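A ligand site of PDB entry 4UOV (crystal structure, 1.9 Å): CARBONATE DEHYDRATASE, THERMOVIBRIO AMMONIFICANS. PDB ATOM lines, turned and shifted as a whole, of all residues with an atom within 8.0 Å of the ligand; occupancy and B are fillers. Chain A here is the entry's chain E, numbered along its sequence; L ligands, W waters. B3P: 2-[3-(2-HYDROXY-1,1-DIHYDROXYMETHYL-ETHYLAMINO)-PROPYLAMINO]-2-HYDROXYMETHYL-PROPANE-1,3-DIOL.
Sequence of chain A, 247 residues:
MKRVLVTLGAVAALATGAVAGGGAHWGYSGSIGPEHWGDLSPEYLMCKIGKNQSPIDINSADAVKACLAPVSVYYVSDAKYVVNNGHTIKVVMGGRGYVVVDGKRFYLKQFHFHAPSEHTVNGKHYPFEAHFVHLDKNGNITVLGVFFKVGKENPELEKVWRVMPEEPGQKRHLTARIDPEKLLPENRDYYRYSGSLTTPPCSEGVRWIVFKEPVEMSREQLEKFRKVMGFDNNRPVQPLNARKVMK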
ATOM      1  N   ASN A  84      35.006 -29.407  28.296  1.00  0.00           N
ATOM      2  CA  ASN A  84      33.646 -29.854  28.579  1.00  0.00           C
ATOM      3  C   ASN A  84      33.795 -31.130  29.386  1.00  0.00           C
ATOM      4  O   ASN A  84      34.226 -32.160  28.861  1.00  0.00           O
ATOM      5  CB  ASN A  84      32.905 -30.122  27.252  1.00  0.00           C
ATOM      6  CG  ASN A  84      31.473 -30.589  27.457  1.00  0.00           C
ATOM      7  OD1 ASN A  84      31.137 -31.212  28.461  1.00  0.00           O
ATOM      8  ND2 ASN A  84      30.626 -30.323  26.467  1.00  0.00           N
ATOM      9  N   MET A 164      33.975 -23.325  22.445  1.00  0.00           N
ATOM     10  CA  MET A 164      33.320 -24.224  23.399  1.00  0.00           C
ATOM     11  C   MET A 164      33.400 -25.688  22.956  1.00  0.00           C
ATOM     12  O   MET A 164      32.915 -26.023  21.878  1.00  0.00           O
ATOM     13  CB  MET A 164      31.855 -23.840  23.599  1.00  0.00           C
ATOM     14  CG  MET A 164      31.223 -24.496  24.829  1.00  0.00           C
ATOM     15  SD  MET A 164      29.452 -24.283  25.009  1.00  0.00           S
ATOM     16  CE  MET A 164      29.331 -22.551  25.460  1.00  0.00           C
ATOM     17  N   PRO A 165      34.026 -26.565  23.775  1.00  0.00           N
ATOM     18  CA  PRO A 165      34.050 -28.000  23.469  1.00  0.00           C
ATOM     19  C   PRO A 165      32.639 -28.581  23.513  1.00  0.00           C
ATOM     20  O   PRO A 165      31.953 -28.475  24.526  1.00  0.00           O
ATOM     21  CB  PRO A 165      34.926 -28.591  24.569  1.00  0.00           C
ATOM     22  CG  PRO A 165      35.678 -27.452  25.162  1.00  0.00           C
ATOM     23  CD  PRO A 165      34.812 -26.246  24.983  1.00  0.00           C
ATOM     24  N   GLU A 166      32.217 -29.182  22.397  1.00  0.00           N
ATOM     25  CA  GLU A 166      30.813 -29.568  22.230  1.00  0.00           C
ATOM     26  C   GLU A 166      30.429 -30.912  22.874  1.00  0.00           C
ATOM     27  O   GLU A 166      29.240 -31.185  23.056  1.00  0.00           O
ATOM     28  CB  GLU A 166      30.427 -29.544  20.744  1.00  0.00           C
ATOM     29  CG  GLU A 166      30.219 -28.135  20.198  1.00  0.00           C
ATOM     30  CD  GLU A 166      30.196 -28.065  18.685  1.00  0.00           C
ATOM     31  OE1 GLU A 166      29.690 -29.021  18.046  1.00  0.00           O
ATOM     32  OE2 GLU A 166      30.665 -27.052  18.128  1.00  0.00           O
ATOM     33  N   GLU A 167      31.405 -31.740  23.198  1.00  0.00           N
ATOM     34  CA  GLU A 167      31.135 -33.065  23.752  1.00  0.00           C
ATOM     35  C   GLU A 167      31.895 -33.310  25.044  1.00  0.00           C
ATOM     36  O   GLU A 167      33.034 -32.871  25.182  1.00  0.00           O
ATOM     37  CB  GLU A 167      31.481 -34.161  22.727  1.00  0.00           C
ATOM     38  CG  GLU A 167      30.837 -34.008  21.354  1.00  0.00           C
ATOM     39  CD  GLU A 167      29.331 -34.187  21.352  1.00  0.00           C
ATOM     40  OE1 GLU A 167      28.787 -34.803  22.297  1.00  0.00           O
ATOM     41  OE2 GLU A 167      28.678 -33.699  20.410  1.00  0.00           O
ATOM     42  N   PRO A 168      31.272 -34.014  26.015  1.00  0.00           N
ATOM     43  CA  PRO A 168      31.966 -34.326  27.262  1.00  0.00           C
ATOM     44  C   PRO A 168      33.290 -35.028  27.021  1.00  0.00           C
ATOM     45  O   PRO A 168      33.361 -35.952  26.209  1.00  0.00           O
ATOM     46  CB  PRO A 168      31.003 -35.283  27.975  1.00  0.00           C
ATOM     47  CG  PRO A 168      29.663 -34.859  27.489  1.00  0.00           C
ATOM     48  CD  PRO A 168      29.856 -34.454  26.050  1.00  0.00           C
ATOM     49  N   GLN A 170      35.970 -33.435  25.797  1.00  0.00           N
ATOM     50  CA  GLN A 170      36.738 -32.646  24.828  1.00  0.00           C
ATOM     51  C   GLN A 170      37.386 -31.405  25.455  1.00  0.00           C
ATOM     52  O   GLN A 170      36.788 -30.733  26.297  1.00  0.00           O
ATOM     53  CB  GLN A 170      35.857 -32.209  23.656  1.00  0.00           C
ATOM     54  CG  GLN A 170      35.394 -33.350  22.756  1.00  0.00           C
ATOM     55  CD  GLN A 170      34.510 -32.892  21.605  1.00  0.00           C
ATOM     56  OE1 GLN A 170      34.050 -31.752  21.564  1.00  0.00           O
ATOM     57  NE2 GLN A 170      34.269 -33.791  20.666  1.00  0.00           N
ATOM     58  N   LYS A 224      23.418 -21.252  23.458  1.00  0.00           N
ATOM     59  CA  LYS A 224      24.516 -22.131  23.070  1.00  0.00           C
ATOM     60  C   LYS A 224      24.980 -23.002  24.242  1.00  0.00           C
ATOM     61  O   LYS A 224      25.222 -24.210  24.073  1.00  0.00           O
ATOM     62  CB  LYS A 224      25.693 -21.380  22.472  1.00  0.00           C
ATOM     63  CG  LYS A 224      26.832 -22.315  22.094  1.00  0.00           C
ATOM     64  CD  LYS A 224      27.879 -21.678  21.199  1.00  0.00           C
ATOM     65  CE  LYS A 224      28.967 -22.696  20.890  1.00  0.00           C
ATOM     66  NZ  LYS A 224      30.158 -22.086  20.242  1.00  0.00           N
ATOM     67  N   PHE A 225      25.115 -22.377  25.426  1.00  0.00           N
ATOM     68  CA  PHE A 225      25.475 -23.106  26.639  1.00  0.00           C
ATOM     69  C   PHE A 225      24.451 -24.192  26.976  1.00  0.00           C
ATOM     70  O   PHE A 225      24.825 -25.344  27.181  1.00  0.00           O
ATOM     71  CB  PHE A 225      25.647 -22.164  27.849  1.00  0.00           C
ATOM     72  CG  PHE A 225      26.060 -22.877  29.116  1.00  0.00           C
ATOM     73  CD1 PHE A 225      27.401 -23.240  29.318  1.00  0.00           C
ATOM     74  CD2 PHE A 225      25.124 -23.179  30.094  1.00  0.00           C
ATOM     75  CE1 PHE A 225      27.790 -23.897  30.482  1.00  0.00           C
ATOM     76  CE2 PHE A 225      25.516 -23.825  31.268  1.00  0.00           C
ATOM     77  CZ  PHE A 225      26.853 -24.179  31.460  1.00  0.00           C
ATOM     78  N   ARG A 226      23.161 -23.836  27.013  1.00  0.00           N
ATOM     79  CA  ARG A 226      22.114 -24.804  27.318  1.00  0.00           C
ATOM     80  C   ARG A 226      22.044 -25.940  26.297  1.00  0.00           C
ATOM     81  O   ARG A 226      21.764 -27.083  26.649  1.00  0.00           O
ATOM     82  CB  ARG A 226      20.757 -24.130  27.445  1.00  0.00           C
ATOM     83  CG  ARG A 226      20.624 -23.199  28.646  1.00  0.00           C
ATOM     84  CD  ARG A 226      19.245 -22.572  28.623  1.00  0.00           C
ATOM     85  NE  ARG A 226      18.192 -23.509  29.004  1.00  0.00           N
ATOM     86  CZ  ARG A 226      16.946 -23.456  28.540  1.00  0.00           C
ATOM     87  NH1 ARG A 226      16.612 -22.523  27.656  1.00  0.00           N
ATOM     88  NH2 ARG A 226      16.036 -24.348  28.937  1.00  0.00           N
ATOM     89  N   LYS A 227      22.303 -25.614  25.032  1.00  0.00           N
ATOM     90  CA  LYS A 227      22.268 -26.607  23.966  1.00  0.00           C
ATOM     91  C   LYS A 227      23.423 -27.615  24.103  1.00  0.00           C
ATOM     92  O   LYS A 227      23.209 -28.814  24.036  1.00  0.00           O
ATOM     93  CB  LYS A 227      22.279 -25.927  22.590  1.00  0.00           C
ATOM     94  CG  LYS A 227      22.147 -26.904  21.420  1.00  0.00           C
ATOM     95  CD  LYS A 227      22.528 -26.225  20.104  1.00  0.00           C
ATOM     96  CE  LYS A 227      22.663 -27.234  18.972  1.00  0.00           C
ATOM     97  NZ  LYS A 227      21.330 -27.684  18.481  1.00  0.00           N
ATOM     98  N   VAL A 228      24.634 -27.115  24.327  1.00  0.00           N
ATOM     99  CA  VAL A 228      25.809 -27.960  24.466  1.00  0.00           C
ATOM    100  C   VAL A 228      25.703 -28.844  25.722  1.00  0.00           C
ATOM    101  O   VAL A 228      25.970 -30.046  25.671  1.00  0.00           O
ATOM    102  CB  VAL A 228      27.108 -27.149  24.407  1.00  0.00           C
ATOM    103  CG1 VAL A 228      28.304 -27.939  24.911  1.00  0.00           C
ATOM    104  CG2 VAL A 228      27.360 -26.658  22.972  1.00  0.00           C
ATOM    105  N   MET A 229      25.263 -28.238  26.840  1.00  0.00           N
ATOM    106  CA  MET A 229      25.122 -28.995  28.089  1.00  0.00           C
ATOM    107  C   MET A 229      24.083 -30.087  27.981  1.00  0.00           C
ATOM    108  O   MET A 229      24.352 -31.235  28.356  1.00  0.00           O
ATOM    109  CB  MET A 229      24.788 -28.065  29.272  1.00  0.00           C
ATOM    110  CG  MET A 229      25.948 -27.181  29.725  1.00  0.00           C
ATOM    111  SD  MET A 229      27.332 -28.065  30.463  1.00  0.00           S
ATOM    112  CE  MET A 229      26.472 -29.004  31.737  1.00  0.00           C
ATOM    113  N   GLY A 230      22.894 -29.759  27.475  1.00  0.00           N
ATOM    114  CA  GLY A 230      21.807 -30.706  27.332  1.00  0.00           C
ATOM    115  C   GLY A 230      20.955 -30.891  28.570  1.00  0.00           C
ATOM    116  O   GLY A 230      20.000 -31.649  28.556  1.00  0.00           O
ATOM    117  N   PHE A 231      21.305 -30.177  29.663  1.00  0.00           N
ATOM    118  CA  PHE A 231      20.536 -30.272  30.917  1.00  0.00           C
ATOM    119  C   PHE A 231      20.852 -29.094  31.860  1.00  0.00           C
ATOM    120  O   PHE A 231      21.925 -28.489  31.732  1.00  0.00           O
ATOM    121  CB  PHE A 231      20.789 -31.611  31.645  1.00  0.00           C
ATOM    122  CG  PHE A 231      22.246 -31.953  31.843  1.00  0.00           C
ATOM    123  CD1 PHE A 231      22.986 -31.403  32.903  1.00  0.00           C
ATOM    124  CD2 PHE A 231      22.861 -32.865  30.990  1.00  0.00           C
ATOM    125  CE1 PHE A 231      24.331 -31.726  33.068  1.00  0.00           C
ATOM    126  CE2 PHE A 231      24.201 -33.199  31.169  1.00  0.00           C
ATOM    127  CZ  PHE A 231      24.937 -32.630  32.197  1.00  0.00           C
HETATM  128  C1  B3P L   1      22.886 -33.138  24.405  1.00  0.00           C
HETATM  129  C2  B3P L   1      24.085 -32.374  23.840  1.00  0.00           C
HETATM  130  C3  B3P L   1      23.087 -34.656  24.392  1.00  0.00           C
HETATM  131  N1  B3P L   1      21.830 -35.404  24.409  1.00  0.00           N
HETATM  132  C4  B3P L   1      21.740 -36.865  24.570  1.00  0.00           C
HETATM  133  C5  B3P L   1      20.493 -37.183  25.412  1.00  0.00           C
HETATM  134  C6  B3P L   1      21.575 -37.599  23.234  1.00  0.00           C
HETATM  135  C7  B3P L   1      23.002 -37.390  25.298  1.00  0.00           C
HETATM  136  N2  B3P L   1      24.279 -32.552  22.411  1.00  0.00           N
HETATM  137  C8  B3P L   1      25.105 -31.672  21.584  1.00  0.00           C
HETATM  138  C9  B3P L   1      25.422 -32.417  20.288  1.00  0.00           C
HETATM  139  C10 B3P L   1      24.344 -30.381  21.251  1.00  0.00           C
HETATM  140  C11 B3P L   1      26.397 -31.349  22.327  1.00  0.00           C
HETATM  141  O1  B3P L   1      26.259 -33.553  20.547  1.00  0.00           O
HETATM  142  O2  B3P L   1      23.003 -30.688  20.850  1.00  0.00           O
HETATM  143  O3  B3P L   1      27.095 -30.233  21.771  1.00  0.00           O
HETATM  144  O4  B3P L   1      19.302 -36.594  24.877  1.00  0.00           O
HETATM  145  O5  B3P L   1      22.549 -37.192  22.266  1.00  0.00           O
HETATM  146  O6  B3P L   1      23.044 -36.959  26.671  1.00  0.00           O
HETATM  147  O   HOH W   1      24.344 -34.161  27.427  1.00  0.00           O
HETATM  148  O   HOH W   2      21.813 -34.275  27.304  1.00  0.00           O
HETATM  149  O   HOH W   3      21.666 -37.219  19.815  1.00  0.00           O
HETATM  150  O   HOH W   4      20.324 -30.683  20.518  1.00  0.00           O
HETATM  151  O   HOH W   5      21.798 -31.040  18.032  1.00  0.00           O
HETATM  152  O   HOH W   6      26.512 -34.242  25.447  1.00  0.00           O
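O of Glu 166 sits at hydrogen-bond distance from O3 of the ligand. The side-chain carboxylate (OE2) of Glu 167 sits at hydrogen-bond distance from an oxygen (O1) of the ligand (2.4 Å).
The side-chain amide oxygen (OE1) of Gln 170 lies within hydrogen-bond range of the backbone NH (N) of Glu 167. The backbone NH (N) of Glu 166 sits at hydrogen-bond distance from the side-chain amide oxygen (OE1) of Gln 170.
Lys 227 touches the ligand. Val 228 touches the ligand. Gly 230 touches the ligand (CA to C1, 3.96 Å). Hydrophobic or aromatic side chains within 4 Å of the ligand: Val 228. Five residues have an atom within 4 Å of the ligand: Glu 166, Glu 167, Lys 227, Val 228 and Gly 230. Along chain A the residues within 4 Å of the ligand span positions 166 to 230. The nearest printed residue that does not touch the ligand is Met 229 (4.6 Å).
Water W2 lies within hydrogen-bond range of an oxygen (O6) of the ligand (3.0 Å) and the backbone carbonyl oxygen of Gly 230 (3.4 Å). Water W5 bridges an oxygen (O2) of the ligand (3.1 Å) and the side-chain amino group of Lys 227 (3.4 Å). Water W1 bridges O of Met 229 and O6 of the ligand.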
